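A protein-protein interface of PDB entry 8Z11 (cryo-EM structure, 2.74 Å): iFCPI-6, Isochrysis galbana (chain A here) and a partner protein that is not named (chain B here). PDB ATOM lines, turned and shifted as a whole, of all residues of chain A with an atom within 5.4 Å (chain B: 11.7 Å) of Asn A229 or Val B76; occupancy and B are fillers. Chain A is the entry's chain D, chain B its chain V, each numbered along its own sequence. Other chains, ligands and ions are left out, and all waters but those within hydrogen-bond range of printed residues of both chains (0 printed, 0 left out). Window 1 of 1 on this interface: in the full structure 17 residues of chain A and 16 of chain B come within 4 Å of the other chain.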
ATOM      1  N   SER A 224     -25.387 -18.243  23.164  1.00  0.00           N
ATOM      2  CA  SER A 224     -26.411 -18.322  24.200  1.00  0.00           C
ATOM      3  C   SER A 224     -26.007 -19.305  25.286  1.00  0.00           C
ATOM      4  O   SER A 224     -26.072 -18.989  26.478  1.00  0.00           O
ATOM      5  CB  SER A 224     -27.751 -18.727  23.592  1.00  0.00           C
ATOM      6  OG  SER A 224     -27.752 -20.099  23.242  1.00  0.00           O
ATOM      7  N   THR A 227     -22.784 -17.871  27.249  1.00  0.00           N
ATOM      8  CA  THR A 227     -22.951 -16.678  28.070  1.00  0.00           C
ATOM      9  C   THR A 227     -24.041 -16.832  29.121  1.00  0.00           C
ATOM     10  O   THR A 227     -23.878 -16.356  30.248  1.00  0.00           O
ATOM     11  CB  THR A 227     -23.283 -15.476  27.186  1.00  0.00           C
ATOM     12  OG1 THR A 227     -24.495 -15.731  26.465  1.00  0.00           O
ATOM     13  CG2 THR A 227     -22.168 -15.198  26.203  1.00  0.00           C
ATOM     14  N   GLY A 228     -25.153 -17.479  28.780  1.00  0.00           N
ATOM     15  CA  GLY A 228     -26.296 -17.497  29.665  1.00  0.00           C
ATOM     16  C   GLY A 228     -27.083 -16.208  29.662  1.00  0.00           C
ATOM     17  O   GLY A 228     -27.659 -15.846  30.690  1.00  0.00           O
ATOM     18  N   ASN A 229     -27.102 -15.492  28.539  1.00  0.00           N
ATOM     19  CA  ASN A 229     -27.818 -14.235  28.378  1.00  0.00           C
ATOM     20  C   ASN A 229     -28.828 -14.371  27.245  1.00  0.00           C
ATOM     21  O   ASN A 229     -28.654 -15.175  26.327  1.00  0.00           O
ATOM     22  CB  ASN A 229     -26.838 -13.094  28.104  1.00  0.00           C
ATOM     23  CG  ASN A 229     -25.912 -12.838  29.277  1.00  0.00           C
ATOM     24  OD1 ASN A 229     -26.345 -12.813  30.428  1.00  0.00           O
ATOM     25  ND2 ASN A 229     -24.629 -12.663  28.993  1.00  0.00           N
ATOM     26  N   GLN A 230     -29.898 -13.575  27.312  1.00  0.00           N
ATOM     27  CA  GLN A 230     -31.117 -13.966  26.604  1.00  0.00           C
ATOM     28  C   GLN A 230     -31.080 -13.624  25.116  1.00  0.00           C
ATOM     29  O   GLN A 230     -30.932 -14.518  24.280  1.00  0.00           O
ATOM     30  CB  GLN A 230     -32.330 -13.309  27.271  1.00  0.00           C
ATOM     31  CG  GLN A 230     -32.877 -14.082  28.461  1.00  0.00           C
ATOM     32  CD  GLN A 230     -33.651 -15.325  28.062  1.00  0.00           C
ATOM     33  OE1 GLN A 230     -34.082 -15.465  26.918  1.00  0.00           O
ATOM     34  NE2 GLN A 230     -33.827 -16.237  29.009  1.00  0.00           N
ATOM     35  N   PHE A 231     -31.207 -12.332  24.759  1.00  0.00           N
ATOM     36  CA  PHE A 231     -31.225 -11.989  23.335  1.00  0.00           C
ATOM     37  C   PHE A 231     -29.855 -11.717  22.722  1.00  0.00           C
ATOM     38  O   PHE A 231     -29.522 -12.329  21.703  1.00  0.00           O
ATOM     39  CB  PHE A 231     -32.109 -10.778  23.044  1.00  0.00           C
ATOM     40  CG  PHE A 231     -31.894 -10.213  21.665  1.00  0.00           C
ATOM     41  CD1 PHE A 231     -32.172 -10.978  20.540  1.00  0.00           C
ATOM     42  CD2 PHE A 231     -31.394  -8.936  21.491  1.00  0.00           C
ATOM     43  CE1 PHE A 231     -31.964 -10.473  19.273  1.00  0.00           C
ATOM     44  CE2 PHE A 231     -31.186  -8.426  20.223  1.00  0.00           C
ATOM     45  CZ  PHE A 231     -31.471  -9.196  19.114  1.00  0.00           C
ATOM     46  N   PRO A 232     -29.042 -10.805  23.268  1.00  0.00           N
ATOM     47  CA  PRO A 232     -27.844 -10.392  22.522  1.00  0.00           C
ATOM     48  C   PRO A 232     -26.776 -11.461  22.464  1.00  0.00           C
ATOM     49  O   PRO A 232     -25.945 -11.428  21.549  1.00  0.00           O
ATOM     50  CB  PRO A 232     -27.352  -9.154  23.289  1.00  0.00           C
ATOM     51  CG  PRO A 232     -28.459  -8.797  24.232  1.00  0.00           C
ATOM     52  CD  PRO A 232     -29.120 -10.091  24.553  1.00  0.00           C
ATOM     53  N   TYR A 233     -26.788 -12.415  23.389  1.00  0.00           N
ATOM     54  CA  TYR A 233     -25.737 -13.416  23.509  1.00  0.00           C
ATOM     55  C   TYR A 233     -24.376 -12.735  23.646  1.00  0.00           C
ATOM     56  O   TYR A 233     -23.481 -12.883  22.814  1.00  0.00           O
ATOM     57  CB  TYR A 233     -25.763 -14.386  22.324  1.00  0.00           C
ATOM     58  CG  TYR A 233     -27.140 -14.702  21.796  1.00  0.00           C
ATOM     59  CD1 TYR A 233     -28.062 -15.377  22.575  1.00  0.00           C
ATOM     60  CD2 TYR A 233     -27.509 -14.341  20.510  1.00  0.00           C
ATOM     61  CE1 TYR A 233     -29.314 -15.679  22.093  1.00  0.00           C
ATOM     62  CE2 TYR A 233     -28.761 -14.638  20.021  1.00  0.00           C
ATOM     63  CZ  TYR A 233     -29.662 -15.301  20.821  1.00  0.00           C
ATOM     64  OH  TYR A 233     -30.913 -15.602  20.343  1.00  0.00           O
ATOM     65  N   LEU A 234     -24.249 -11.955  24.716  1.00  0.00           N
ATOM     66  CA  LEU A 234     -23.034 -11.215  25.019  1.00  0.00           C
ATOM     67  C   LEU A 234     -22.711 -11.385  26.492  1.00  0.00           C
ATOM     68  O   LEU A 234     -23.613 -11.413  27.331  1.00  0.00           O
ATOM     69  CB  LEU A 234     -23.185  -9.723  24.693  1.00  0.00           C
ATOM     70  CG  LEU A 234     -23.482  -9.366  23.237  1.00  0.00           C
ATOM     71  CD1 LEU A 234     -23.859  -7.901  23.117  1.00  0.00           C
ATOM     72  CD2 LEU A 234     -22.294  -9.683  22.352  1.00  0.00           C
ATOM     73  N   PHE A 235     -21.421 -11.494  26.801  1.00  0.00           N
ATOM     74  CA  PHE A 235     -21.002 -11.565  28.190  1.00  0.00           C
ATOM     75  C   PHE A 235     -21.370 -10.273  28.914  1.00  0.00           C
ATOM     76  O   PHE A 235     -21.595  -9.226  28.302  1.00  0.00           O
ATOM     77  CB  PHE A 235     -19.498 -11.809  28.289  1.00  0.00           C
ATOM     78  CG  PHE A 235     -19.071 -13.176  27.841  1.00  0.00           C
ATOM     79  CD1 PHE A 235     -19.364 -14.291  28.605  1.00  0.00           C
ATOM     80  CD2 PHE A 235     -18.369 -13.345  26.662  1.00  0.00           C
ATOM     81  CE1 PHE A 235     -18.964 -15.549  28.200  1.00  0.00           C
ATOM     82  CE2 PHE A 235     -17.972 -14.600  26.251  1.00  0.00           C
ATOM     83  CZ  PHE A 235     -18.271 -15.703  27.021  1.00  0.00           C
ATOM     84  N   ASP A 236     -21.437 -10.364  30.244  1.00  0.00           N
ATOM     85  CA  ASP A 236     -21.856  -9.218  31.044  1.00  0.00           C
ATOM     86  C   ASP A 236     -20.888  -8.049  30.892  1.00  0.00           C
ATOM     87  O   ASP A 236     -21.309  -6.887  30.862  1.00  0.00           O
ATOM     88  CB  ASP A 236     -21.985  -9.624  32.513  1.00  0.00           C
ATOM     89  CG  ASP A 236     -20.680 -10.129  33.097  1.00  0.00           C
ATOM     90  OD1 ASP A 236     -19.823 -10.599  32.320  1.00  0.00           O
ATOM     91  OD2 ASP A 236     -20.512 -10.056  34.332  1.00  0.00           O
ATOM     92  N   THR A 239     -21.309  -5.466  27.835  1.00  0.00           N
ATOM     93  CA  THR A 239     -22.332  -4.430  27.845  1.00  0.00           C
ATOM     94  C   THR A 239     -21.838  -3.136  28.483  1.00  0.00           C
ATOM     95  O   THR A 239     -22.654  -2.321  28.925  1.00  0.00           O
ATOM     96  CB  THR A 239     -23.580  -4.931  28.574  1.00  0.00           C
ATOM     97  OG1 THR A 239     -23.326  -4.980  29.984  1.00  0.00           O
ATOM     98  CG2 THR A 239     -23.972  -6.317  28.081  1.00  0.00           C
ATOM     99  N   ALA B  71     -41.689 -13.182  27.194  1.00  0.00           N
ATOM    100  CA  ALA B  71     -40.803 -14.191  27.750  1.00  0.00           C
ATOM    101  C   ALA B  71     -40.112 -13.662  29.001  1.00  0.00           C
ATOM    102  O   ALA B  71     -39.939 -12.455  29.185  1.00  0.00           O
ATOM    103  CB  ALA B  71     -39.761 -14.625  26.721  1.00  0.00           C
ATOM    104  N   THR B  72     -39.713 -14.592  29.864  1.00  0.00           N
ATOM    105  CA  THR B  72     -39.048 -14.237  31.111  1.00  0.00           C
ATOM    106  C   THR B  72     -37.660 -13.676  30.839  1.00  0.00           C
ATOM    107  O   THR B  72     -36.767 -14.403  30.395  1.00  0.00           O
ATOM    108  CB  THR B  72     -38.944 -15.454  32.033  1.00  0.00           C
ATOM    109  OG1 THR B  72     -38.171 -16.477  31.390  1.00  0.00           O
ATOM    110  CG2 THR B  72     -40.325 -15.999  32.369  1.00  0.00           C
ATOM    111  N   LYS B  73     -37.468 -12.386  31.102  1.00  0.00           N
ATOM    112  CA  LYS B  73     -36.154 -11.775  30.975  1.00  0.00           C
ATOM    113  C   LYS B  73     -35.308 -12.156  32.181  1.00  0.00           C
ATOM    114  O   LYS B  73     -35.583 -11.729  33.306  1.00  0.00           O
ATOM    115  CB  LYS B  73     -36.276 -10.253  30.859  1.00  0.00           C
ATOM    116  CG  LYS B  73     -37.174  -9.740  29.718  1.00  0.00           C
ATOM    117  CD  LYS B  73     -36.727 -10.177  28.310  1.00  0.00           C
ATOM    118  CE  LYS B  73     -37.899 -10.530  27.398  1.00  0.00           C
ATOM    119  NZ  LYS B  73     -39.036  -9.571  27.478  1.00  0.00           N
ATOM    120  N   LYS B  74     -34.278 -12.964  31.939  1.00  0.00           N
ATOM    121  CA  LYS B  74     -33.474 -13.563  32.996  1.00  0.00           C
ATOM    122  C   LYS B  74     -32.373 -12.622  33.488  1.00  0.00           C
ATOM    123  O   LYS B  74     -31.668 -12.958  34.445  1.00  0.00           O
ATOM    124  CB  LYS B  74     -32.904 -14.895  32.484  1.00  0.00           C
ATOM    125  CG  LYS B  74     -32.141 -15.774  33.487  1.00  0.00           C
ATOM    126  CD  LYS B  74     -31.421 -16.912  32.782  1.00  0.00           C
ATOM    127  CE  LYS B  74     -30.101 -16.465  32.185  1.00  0.00           C
ATOM    128  NZ  LYS B  74     -28.961 -16.690  33.116  1.00  0.00           N
ATOM    129  N   SER B  75     -32.229 -11.441  32.875  1.00  0.00           N
ATOM    130  CA  SER B  75     -31.267 -10.430  33.302  1.00  0.00           C
ATOM    131  C   SER B  75     -29.837 -10.857  32.994  1.00  0.00           C
ATOM    132  O   SER B  75     -29.506 -12.045  33.049  1.00  0.00           O
ATOM    133  CB  SER B  75     -31.413 -10.123  34.796  1.00  0.00           C
ATOM    134  OG  SER B  75     -30.610 -10.997  35.570  1.00  0.00           O
ATOM    135  N   VAL B  76     -28.986  -9.888  32.674  1.00  0.00           N
ATOM    136  CA  VAL B  76     -27.598 -10.154  32.316  1.00  0.00           C
ATOM    137  C   VAL B  76     -26.807 -10.381  33.595  1.00  0.00           C
ATOM    138  O   VAL B  76     -26.902  -9.592  34.543  1.00  0.00           O
ATOM    139  CB  VAL B  76     -26.999  -9.001  31.489  1.00  0.00           C
ATOM    140  CG1 VAL B  76     -25.800  -9.490  30.697  1.00  0.00           C
ATOM    141  CG2 VAL B  76     -28.034  -8.411  30.530  1.00  0.00           C
ATOM    142  N   GLY B  77     -26.030 -11.462  33.626  1.00  0.00           N
ATOM    143  CA  GLY B  77     -25.333 -11.868  34.823  1.00  0.00           C
ATOM    144  C   GLY B  77     -24.066 -12.646  34.521  1.00  0.00           C
ATOM    145  O   GLY B  77     -23.576 -12.652  33.388  1.00  0.00           O
ATOM    146  N   PRO B  78     -23.500 -13.310  35.531  1.00  0.00           N
ATOM    147  CA  PRO B  78     -22.250 -14.046  35.312  1.00  0.00           C
ATOM    148  C   PRO B  78     -22.446 -15.240  34.392  1.00  0.00           C
ATOM    149  O   PRO B  78     -23.538 -15.805  34.287  1.00  0.00           O
ATOM    150  CB  PRO B  78     -21.847 -14.490  36.722  1.00  0.00           C
ATOM    151  CG  PRO B  78     -23.122 -14.556  37.470  1.00  0.00           C
ATOM    152  CD  PRO B  78     -23.975 -13.452  36.920  1.00  0.00           C
ATOM    153  N   LYS B  79     -21.361 -15.619  33.721  1.00  0.00           N
ATOM    154  CA  LYS B  79     -21.404 -16.731  32.790  1.00  0.00           C
ATOM    155  C   LYS B  79     -21.498 -18.055  33.550  1.00  0.00           C
ATOM    156  O   LYS B  79     -21.191 -18.114  34.742  1.00  0.00           O
ATOM    157  CB  LYS B  79     -20.163 -16.721  31.897  1.00  0.00           C
ATOM    158  CG  LYS B  79     -18.838 -16.952  32.632  1.00  0.00           C
ATOM    159  CD  LYS B  79     -17.649 -16.890  31.686  1.00  0.00           C
ATOM    160  CE  LYS B  79     -17.235 -15.456  31.400  1.00  0.00           C
ATOM    161  NZ  LYS B  79     -16.079 -15.384  30.464  1.00  0.00           N
ATOM    162  N   PRO B  80     -21.919 -19.132  32.888  1.00  0.00           N
ATOM    163  CA  PRO B  80     -21.826 -20.460  33.495  1.00  0.00           C
ATOM    164  C   PRO B  80     -20.441 -21.047  33.245  1.00  0.00           C
ATOM    165  O   PRO B  80     -19.600 -20.445  32.580  1.00  0.00           O
ATOM    166  CB  PRO B  80     -22.919 -21.258  32.778  1.00  0.00           C
ATOM    167  CG  PRO B  80     -23.235 -20.489  31.522  1.00  0.00           C
ATOM    168  CD  PRO B  80     -22.419 -19.230  31.507  1.00  0.00           C
ATOM    169  N   GLU B  81     -20.221 -22.242  33.787  1.00  0.00           N
ATOM    170  CA  GLU B  81     -18.968 -22.963  33.622  1.00  0.00           C
ATOM    171  C   GLU B  81     -19.104 -24.028  32.539  1.00  0.00           C
ATOM    172  O   GLU B  81     -20.168 -24.637  32.357  1.00  0.00           O
ATOM    173  CB  GLU B  81     -18.529 -23.611  34.942  1.00  0.00           C
ATOM    174  CG  GLU B  81     -17.096 -24.183  34.995  1.00  0.00           C
ATOM    175  CD  GLU B  81     -16.029 -23.265  34.420  1.00  0.00           C
ATOM    176  OE1 GLU B  81     -15.111 -23.769  33.741  1.00  0.00           O
ATOM    177  OE2 GLU B  81     -16.110 -22.039  34.650  1.00  0.00           O
ATOM    178  N   PHE B  85     -22.240 -26.796  31.964  1.00  0.00           N
ATOM    179  CA  PHE B  85     -23.120 -27.107  30.838  1.00  0.00           C
ATOM    180  C   PHE B  85     -22.565 -28.197  29.920  1.00  0.00           C
ATOM    181  O   PHE B  85     -23.135 -28.427  28.849  1.00  0.00           O
ATOM    182  CB  PHE B  85     -23.477 -25.841  30.038  1.00  0.00           C
ATOM    183  CG  PHE B  85     -22.317 -25.132  29.381  1.00  0.00           C
ATOM    184  CD1 PHE B  85     -21.748 -25.607  28.210  1.00  0.00           C
ATOM    185  CD2 PHE B  85     -21.857 -23.931  29.894  1.00  0.00           C
ATOM    186  CE1 PHE B  85     -20.711 -24.936  27.605  1.00  0.00           C
ATOM    187  CE2 PHE B  85     -20.824 -23.252  29.285  1.00  0.00           C
ATOM    188  CZ  PHE B  85     -20.254 -23.753  28.135  1.00  0.00           C
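Of the 12 printed residues of chain A, 6 touch a printed residue of chain B.
Of the 12 printed residues of chain B, 6 touch a printed residue of chain A.
Hydrophobic or aromatic side chains of chain B that line the printed part of chain A: Val B76 and Pro B80.
Among the printed residues, 10 pairs touch across the chains.
Of the printed residues of chain B, Asn A229 touches Val B76 and Gly B77.
Val B76 touches two residues of chain A.
No residue of chain B comes within 4 Å of Ser A224.
Gly A228 touches just one residue of chain B: Lys B74.
Gln A230 touches two residues of chain B.
No residue of chain B comes within 4 Å of Pro A232.
No residue of chain B comes within 4 Å of Tyr A233.
No residue of chain B comes within 4 Å of Leu A234.
Phe A235 touches just one residue of chain B: Lys B79 (3.6 Å).
Asp A236 touches just these residues of chain B: Val B76 and Gly B77.
Of the printed residues of chain B, Thr A227 touches Lys B79 and Pro B80.
Of the printed residues of chain A, Lys B79 touches Thr A227 (3.6 Å) and Phe A235 (3.6 Å).
Of the printed residues of chain A, Thr B72 touches Gln A230.
Of the printed residues of chain A, Pro B80 touches Thr A227.
Glu B81 touches none of the printed residues of chain A.
The nearest residue of chain B that does not touch Asn A229 is Ser B75 (4.2 Å).
Among the printed residues, pairs that only touch across the chains: Asn A229 with Val B76 (3.4 Å), Thr A227 with Pro B80 (3.5 Å), Asp A236 with Gly B77 (3.5 Å), Thr A227 with Lys B79 (3.6 Å), Phe A235 with Lys B79 (3.6 Å), Gln A230 with Thr B72 (3.7 Å), Gln A230 with Lys B74 (3.8 Å) and Asp A236 with Val B76 (3.97 Å).
The backbone carbonyl oxygen (O) of Asp A236 sits at hydrogen-bond distance from the side-chain hydroxyl (OG1) of Thr A239.
The side-chain hydroxyl (OG1) of Thr A227 is in hydrogen-bond range of the backbone NH (N) of Asn A229, 3.3 Å away.
The side-chain amide oxygen of Asn A229 sits at hydrogen-bond distance from the backbone NH of Gly B77 (3.5 Å).
O of Gly A228 lies within hydrogen-bond range of NZ of Lys B74, 2.9 Å away.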
